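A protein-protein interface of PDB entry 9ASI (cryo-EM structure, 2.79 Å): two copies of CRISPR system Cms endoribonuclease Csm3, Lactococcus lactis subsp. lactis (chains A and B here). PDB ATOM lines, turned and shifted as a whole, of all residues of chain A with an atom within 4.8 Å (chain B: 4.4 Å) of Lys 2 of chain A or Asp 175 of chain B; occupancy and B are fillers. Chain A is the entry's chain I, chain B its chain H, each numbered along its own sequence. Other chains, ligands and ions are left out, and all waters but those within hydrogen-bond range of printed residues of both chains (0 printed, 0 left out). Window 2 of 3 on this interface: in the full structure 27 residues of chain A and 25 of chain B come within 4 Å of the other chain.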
ATOM      1  N   MET A   1      28.277  25.983 -25.537  1.00  0.00           N
ATOM      2  CA  MET A   1      28.182  24.600 -25.980  1.00  0.00           C
ATOM      3  C   MET A   1      26.727  24.155 -26.078  1.00  0.00           C
ATOM      4  O   MET A   1      25.812  24.975 -26.026  1.00  0.00           O
ATOM      5  CB  MET A   1      28.953  23.680 -25.034  1.00  0.00           C
ATOM      6  CG  MET A   1      30.429  24.018 -24.915  1.00  0.00           C
ATOM      7  SD  MET A   1      31.447  22.590 -24.497  1.00  0.00           S
ATOM      8  CE  MET A   1      31.535  21.762 -26.081  1.00  0.00           C
ATOM      9  N   LYS A   2      26.523  22.852 -26.230  1.00  0.00           N
ATOM     10  CA  LYS A   2      25.202  22.256 -26.406  1.00  0.00           C
ATOM     11  C   LYS A   2      25.051  21.030 -25.517  1.00  0.00           C
ATOM     12  O   LYS A   2      24.738  19.929 -25.972  1.00  0.00           O
ATOM     13  CB  LYS A   2      24.931  21.919 -27.868  1.00  0.00           C
ATOM     14  CG  LYS A   2      23.455  21.681 -28.181  1.00  0.00           C
ATOM     15  CD  LYS A   2      22.547  22.688 -27.486  1.00  0.00           C
ATOM     16  CE  LYS A   2      22.615  24.058 -28.136  1.00  0.00           C
ATOM     17  NZ  LYS A   2      21.751  25.042 -27.438  1.00  0.00           N
ATOM     18  N   LEU A   3      25.336  21.200 -24.230  1.00  0.00           N
ATOM     19  CA  LEU A   3      25.144  20.126 -23.265  1.00  0.00           C
ATOM     20  C   LEU A   3      23.700  19.632 -23.296  1.00  0.00           C
ATOM     21  O   LEU A   3      22.760  20.420 -23.428  1.00  0.00           O
ATOM     22  CB  LEU A   3      25.509  20.614 -21.864  1.00  0.00           C
ATOM     23  CG  LEU A   3      26.988  20.704 -21.494  1.00  0.00           C
ATOM     24  CD1 LEU A   3      27.691  21.811 -22.243  1.00  0.00           C
ATOM     25  CD2 LEU A   3      27.109  20.943 -20.019  1.00  0.00           C
ATOM     26  N   VAL A   4      23.527  18.317 -23.185  1.00  0.00           N
ATOM     27  CA  VAL A   4      22.222  17.668 -23.293  1.00  0.00           C
ATOM     28  C   VAL A   4      21.923  16.985 -21.966  1.00  0.00           C
ATOM     29  O   VAL A   4      22.581  16.000 -21.608  1.00  0.00           O
ATOM     30  CB  VAL A   4      22.178  16.659 -24.446  1.00  0.00           C
ATOM     31  CG1 VAL A   4      20.890  15.861 -24.401  1.00  0.00           C
ATOM     32  CG2 VAL A   4      22.333  17.367 -25.782  1.00  0.00           C
ATOM     33  N   LYS A  95      16.639  24.424 -22.762  1.00  0.00           N
ATOM     34  CA  LYS A  95      15.683  24.163 -23.833  1.00  0.00           C
ATOM     35  C   LYS A  95      14.920  22.897 -23.458  1.00  0.00           C
ATOM     36  O   LYS A  95      15.332  21.784 -23.787  1.00  0.00           O
ATOM     37  CB  LYS A  95      16.387  24.022 -25.178  1.00  0.00           C
ATOM     38  CG  LYS A  95      15.490  24.218 -26.386  1.00  0.00           C
ATOM     39  CD  LYS A  95      14.826  22.922 -26.800  1.00  0.00           C
ATOM     40  CE  LYS A  95      13.889  23.145 -27.963  1.00  0.00           C
ATOM     41  NZ  LYS A  95      12.952  22.020 -28.187  1.00  0.00           N
ATOM     42  N   PHE A 149      18.082  20.317 -23.524  1.00  0.00           N
ATOM     43  CA  PHE A 149      19.319  20.883 -24.041  1.00  0.00           C
ATOM     44  C   PHE A 149      19.776  22.043 -23.162  1.00  0.00           C
ATOM     45  O   PHE A 149      18.987  22.667 -22.450  1.00  0.00           O
ATOM     46  CB  PHE A 149      19.141  21.345 -25.488  1.00  0.00           C
ATOM     47  CG  PHE A 149      18.689  20.257 -26.420  1.00  0.00           C
ATOM     48  CD1 PHE A 149      19.062  18.945 -26.205  1.00  0.00           C
ATOM     49  CD2 PHE A 149      17.884  20.546 -27.505  1.00  0.00           C
ATOM     50  CE1 PHE A 149      18.645  17.945 -27.056  1.00  0.00           C
ATOM     51  CE2 PHE A 149      17.464  19.546 -28.357  1.00  0.00           C
ATOM     52  CZ  PHE A 149      17.848  18.245 -28.132  1.00  0.00           C
ATOM     53  N   TYR A 150      21.076  22.324 -23.212  1.00  0.00           N
ATOM     54  CA  TYR A 150      21.665  23.387 -22.412  1.00  0.00           C
ATOM     55  C   TYR A 150      22.656  24.171 -23.260  1.00  0.00           C
ATOM     56  O   TYR A 150      23.309  23.620 -24.148  1.00  0.00           O
ATOM     57  CB  TYR A 150      22.363  22.834 -21.164  1.00  0.00           C
ATOM     58  CG  TYR A 150      23.063  23.887 -20.340  1.00  0.00           C
ATOM     59  CD1 TYR A 150      22.358  24.687 -19.458  1.00  0.00           C
ATOM     60  CD2 TYR A 150      24.429  24.081 -20.446  1.00  0.00           C
ATOM     61  CE1 TYR A 150      22.993  25.650 -18.706  1.00  0.00           C
ATOM     62  CE2 TYR A 150      25.073  25.037 -19.699  1.00  0.00           C
ATOM     63  CZ  TYR A 150      24.351  25.820 -18.830  1.00  0.00           C
ATOM     64  OH  TYR A 150      24.992  26.780 -18.084  1.00  0.00           O
ATOM     65  N   ASN A 151      22.756  25.466 -22.973  1.00  0.00           N
ATOM     66  CA  ASN A 151      23.665  26.375 -23.661  1.00  0.00           C
ATOM     67  C   ASN A 151      24.758  26.805 -22.694  1.00  0.00           C
ATOM     68  O   ASN A 151      24.465  27.396 -21.651  1.00  0.00           O
ATOM     69  CB  ASN A 151      22.916  27.599 -24.184  1.00  0.00           C
ATOM     70  CG  ASN A 151      22.605  27.509 -25.657  1.00  0.00           C
ATOM     71  OD1 ASN A 151      23.263  26.781 -26.398  1.00  0.00           O
ATOM     72  ND2 ASN A 151      21.598  28.254 -26.094  1.00  0.00           N
ATOM     73  N   ILE A 196      25.347  14.996 -21.234  1.00  0.00           N
ATOM     74  CA  ILE A 196      26.365  14.703 -22.232  1.00  0.00           C
ATOM     75  C   ILE A 196      26.484  15.906 -23.158  1.00  0.00           C
ATOM     76  O   ILE A 196      25.581  16.742 -23.249  1.00  0.00           O
ATOM     77  CB  ILE A 196      26.044  13.421 -23.034  1.00  0.00           C
ATOM     78  CG1 ILE A 196      27.330  12.761 -23.533  1.00  0.00           C
ATOM     79  CG2 ILE A 196      25.107  13.725 -24.192  1.00  0.00           C
ATOM     80  N   THR A 197      27.622  16.003 -23.835  1.00  0.00           N
ATOM     81  CA  THR A 197      27.843  17.059 -24.810  1.00  0.00           C
ATOM     82  C   THR A 197      27.320  16.616 -26.169  1.00  0.00           C
ATOM     83  O   THR A 197      27.525  15.473 -26.584  1.00  0.00           O
ATOM     84  CB  THR A 197      29.329  17.414 -24.911  1.00  0.00           C
ATOM     85  OG1 THR A 197      29.885  17.534 -23.599  1.00  0.00           O
ATOM     86  CG2 THR A 197      29.507  18.732 -25.635  1.00  0.00           C
ATOM     87  N   ALA A 198      26.624  17.527 -26.853  1.00  0.00           N
ATOM     88  CA  ALA A 198      26.070  17.198 -28.162  1.00  0.00           C
ATOM     89  C   ALA A 198      27.175  16.936 -29.177  1.00  0.00           C
ATOM     90  O   ALA A 198      27.154  15.928 -29.891  1.00  0.00           O
ATOM     91  CB  ALA A 198      25.156  18.324 -28.642  1.00  0.00           C
ATOM     92  N   LYS B  52      17.530  30.729 -38.637  1.00  0.00           N
ATOM     93  CA  LYS B  52      17.962  29.937 -37.494  1.00  0.00           C
ATOM     94  C   LYS B  52      19.264  29.203 -37.790  1.00  0.00           C
ATOM     95  O   LYS B  52      20.173  29.175 -36.949  1.00  0.00           O
ATOM     96  CB  LYS B  52      16.861  28.962 -37.095  1.00  0.00           C
ATOM     97  CG  LYS B  52      17.076  28.313 -35.756  1.00  0.00           C
ATOM     98  CD  LYS B  52      17.135  29.352 -34.661  1.00  0.00           C
ATOM     99  CE  LYS B  52      16.944  28.712 -33.309  1.00  0.00           C
ATOM    100  NZ  LYS B  52      17.244  29.631 -32.187  1.00  0.00           N
ATOM    101  N   LEU B  56      22.771  29.918 -35.740  1.00  0.00           N
ATOM    102  CA  LEU B  56      23.489  28.861 -35.038  1.00  0.00           C
ATOM    103  C   LEU B  56      24.881  28.661 -35.618  1.00  0.00           C
ATOM    104  O   LEU B  56      25.859  28.543 -34.872  1.00  0.00           O
ATOM    105  CB  LEU B  56      22.688  27.561 -35.093  1.00  0.00           C
ATOM    106  CG  LEU B  56      21.389  27.557 -34.288  1.00  0.00           C
ATOM    107  CD1 LEU B  56      20.611  26.289 -34.550  1.00  0.00           C
ATOM    108  CD2 LEU B  56      21.687  27.711 -32.813  1.00  0.00           C
ATOM    109  N   LEU B 171      23.449  21.542 -35.770  1.00  0.00           N
ATOM    110  CA  LEU B 171      23.122  22.505 -34.725  1.00  0.00           C
ATOM    111  C   LEU B 171      21.614  22.645 -34.575  1.00  0.00           C
ATOM    112  O   LEU B 171      21.102  22.728 -33.454  1.00  0.00           O
ATOM    113  CB  LEU B 171      23.760  23.859 -35.033  1.00  0.00           C
ATOM    114  CG  LEU B 171      25.285  23.936 -34.948  1.00  0.00           C
ATOM    115  CD1 LEU B 171      25.785  25.170 -35.661  1.00  0.00           C
ATOM    116  CD2 LEU B 171      25.748  23.935 -33.510  1.00  0.00           C
ATOM    117  N   LEU B 172      20.888  22.666 -35.693  1.00  0.00           N
ATOM    118  CA  LEU B 172      19.430  22.679 -35.625  1.00  0.00           C
ATOM    119  C   LEU B 172      18.877  21.442 -34.929  1.00  0.00           C
ATOM    120  O   LEU B 172      17.846  21.521 -34.253  1.00  0.00           O
ATOM    121  CB  LEU B 172      18.838  22.793 -37.027  1.00  0.00           C
ATOM    122  CG  LEU B 172      18.937  24.153 -37.702  1.00  0.00           C
ATOM    123  CD1 LEU B 172      18.558  24.040 -39.155  1.00  0.00           C
ATOM    124  CD2 LEU B 172      17.995  25.097 -36.999  1.00  0.00           C
ATOM    125  N   GLU B 173      19.537  20.292 -35.087  1.00  0.00           N
ATOM    126  CA  GLU B 173      19.038  19.057 -34.491  1.00  0.00           C
ATOM    127  C   GLU B 173      19.071  19.106 -32.970  1.00  0.00           C
ATOM    128  O   GLU B 173      18.237  18.473 -32.314  1.00  0.00           O
ATOM    129  CB  GLU B 173      19.847  17.866 -34.998  1.00  0.00           C
ATOM    130  CG  GLU B 173      19.570  17.513 -36.443  1.00  0.00           C
ATOM    131  CD  GLU B 173      19.639  16.026 -36.698  1.00  0.00           C
ATOM    132  OE1 GLU B 173      19.128  15.256 -35.858  1.00  0.00           O
ATOM    133  OE2 GLU B 173      20.209  15.623 -37.734  1.00  0.00           O
ATOM    134  N   PHE B 174      20.020  19.838 -32.395  1.00  0.00           N
ATOM    135  CA  PHE B 174      20.123  20.014 -30.950  1.00  0.00           C
ATOM    136  C   PHE B 174      19.598  21.371 -30.523  1.00  0.00           C
ATOM    137  O   PHE B 174      20.134  22.013 -29.618  1.00  0.00           O
ATOM    138  CB  PHE B 174      21.560  19.820 -30.494  1.00  0.00           C
ATOM    139  CG  PHE B 174      22.037  18.411 -30.610  1.00  0.00           C
ATOM    140  CD1 PHE B 174      21.788  17.501 -29.603  1.00  0.00           C
ATOM    141  CD2 PHE B 174      22.721  17.991 -31.734  1.00  0.00           C
ATOM    142  CE1 PHE B 174      22.221  16.202 -29.710  1.00  0.00           C
ATOM    143  CE2 PHE B 174      23.154  16.692 -31.848  1.00  0.00           C
ATOM    144  CZ  PHE B 174      22.906  15.795 -30.835  1.00  0.00           C
ATOM    145  N   ASP B 175      18.541  21.820 -31.182  1.00  0.00           N
ATOM    146  CA  ASP B 175      17.940  23.121 -30.946  1.00  0.00           C
ATOM    147  C   ASP B 175      16.504  23.041 -31.457  1.00  0.00           C
ATOM    148  O   ASP B 175      16.005  21.955 -31.771  1.00  0.00           O
ATOM    149  CB  ASP B 175      18.761  24.215 -31.634  1.00  0.00           C
ATOM    150  CG  ASP B 175      18.461  25.588 -31.104  1.00  0.00           C
ATOM    151  OD1 ASP B 175      19.003  25.952 -30.042  1.00  0.00           O
ATOM    152  OD2 ASP B 175      17.666  26.298 -31.741  1.00  0.00           O
ATOM    153  N   TYR B 176      15.839  24.183 -31.557  1.00  0.00           N
ATOM    154  CA  TYR B 176      14.471  24.227 -32.044  1.00  0.00           C
ATOM    155  C   TYR B 176      14.380  25.004 -33.349  1.00  0.00           C
ATOM    156  O   TYR B 176      15.295  25.735 -33.735  1.00  0.00           O
ATOM    157  CB  TYR B 176      13.532  24.842 -31.005  1.00  0.00           C
ATOM    158  CG  TYR B 176      13.940  26.205 -30.513  1.00  0.00           C
ATOM    159  CD1 TYR B 176      14.902  26.348 -29.526  1.00  0.00           C
ATOM    160  CD2 TYR B 176      13.351  27.350 -31.020  1.00  0.00           C
ATOM    161  CE1 TYR B 176      15.272  27.587 -29.068  1.00  0.00           C
ATOM    162  CE2 TYR B 176      13.714  28.596 -30.567  1.00  0.00           C
ATOM    163  CZ  TYR B 176      14.676  28.708 -29.590  1.00  0.00           C
ATOM    164  OH  TYR B 176      15.050  29.948 -29.131  1.00  0.00           O
ATOM    165  N   ARG B 187      11.189  21.173 -31.740  1.00  0.00           N
ATOM    166  CA  ARG B 187      12.238  20.193 -31.990  1.00  0.00           C
ATOM    167  C   ARG B 187      12.044  19.525 -33.347  1.00  0.00           C
ATOM    168  O   ARG B 187      10.923  19.206 -33.746  1.00  0.00           O
ATOM    169  CB  ARG B 187      12.255  19.147 -30.883  1.00  0.00           C
ATOM    170  CG  ARG B 187      13.607  18.521 -30.647  1.00  0.00           C
ATOM    171  CD  ARG B 187      13.484  17.306 -29.757  1.00  0.00           C
ATOM    172  NE  ARG B 187      14.717  16.533 -29.705  1.00  0.00           N
ATOM    173  CZ  ARG B 187      15.074  15.772 -28.680  1.00  0.00           C
ATOM    174  NH1 ARG B 187      14.310  15.653 -27.608  1.00  0.00           N
ATOM    175  NH2 ARG B 187      16.227  15.113 -28.733  1.00  0.00           N
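Among the printed residues, pairs that only touch across the chains: Lys 2 of chain A with Phe 174 of chain B, Val 4 of chain A with Phe 174 of chain B, Lys 95 of chain A with Tyr 176 of chain B, Phe 149 of chain A with Phe 174 of chain B, Phe 149 of chain A with Asp 175 of chain B, Phe 149 of chain A with Arg 187 of chain B and Ala 198 of chain A with Phe 174 of chain B.
The side-chain amino group (NZ) of Lys 2 of chain A is in salt-bridge range of the side-chain carboxylate (OD1) of Asp 175 of chain B (3.9 Å).
Hydrophobic or aromatic side chains of chain A that line the printed part of chain B: Val 4, Phe 149 and Ala 198.
Lys 2 of chain A touches just these residues of chain B: Phe 174 and Asp 175. Of the printed residues of chain B, Val 4 of chain A touches Phe 174. Printed residues of chain B within 4 Å of Phe 149 of chain A: Phe 174, Asp 175 and Arg 187. Printed residues of chain B within 4 Å of Ala 198 of chain A: Phe 174. Leu 171 of chain B touches none of the printed residues of chain A. Of the printed residues of chain A, Phe 174 of chain B touches Lys 2, Val 4, Phe 149 and Ala 198. Asp 175 of chain B touches just these residues of chain A: Lys 2 (3.9 Å) and Phe 149 (3.8 Å). Of the printed residues of chain A, Arg 187 of chain B touches Phe 149 (3.6 Å). The nearest printed residue of chain A that does not touch Phe 174 of chain B is Lys 95 of chain A (6.1 Å).
No position is printed for both chains. Of the 8 pairs that touch across the chains among the printed residues, none has its exchanged pair printed and touching as well.
The side-chain amino group (NZ) of Lys 2 of chain A is in hydrogen-bond range of the side-chain amide oxygen (OD1) of Asn 151 of chain A, 2.5 Å away. The backbone NH (N) of Lys 95 of chain A lies within hydrogen-bond range of the backbone carbonyl oxygen (O) of Phe 149 of chain A, at 2.9 Å. O of Ile 196 of chain A sits at hydrogen-bond distance from N of Val 4 of chain A (2.6 Å). O of Lys 2 of chain A sits close to N of Ala 198 of chain A, 3.2 Å away. NZ of Lys 52 of chain B is in salt-bridge range of OD2 of Asp 175 of chain B (3.4 Å).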
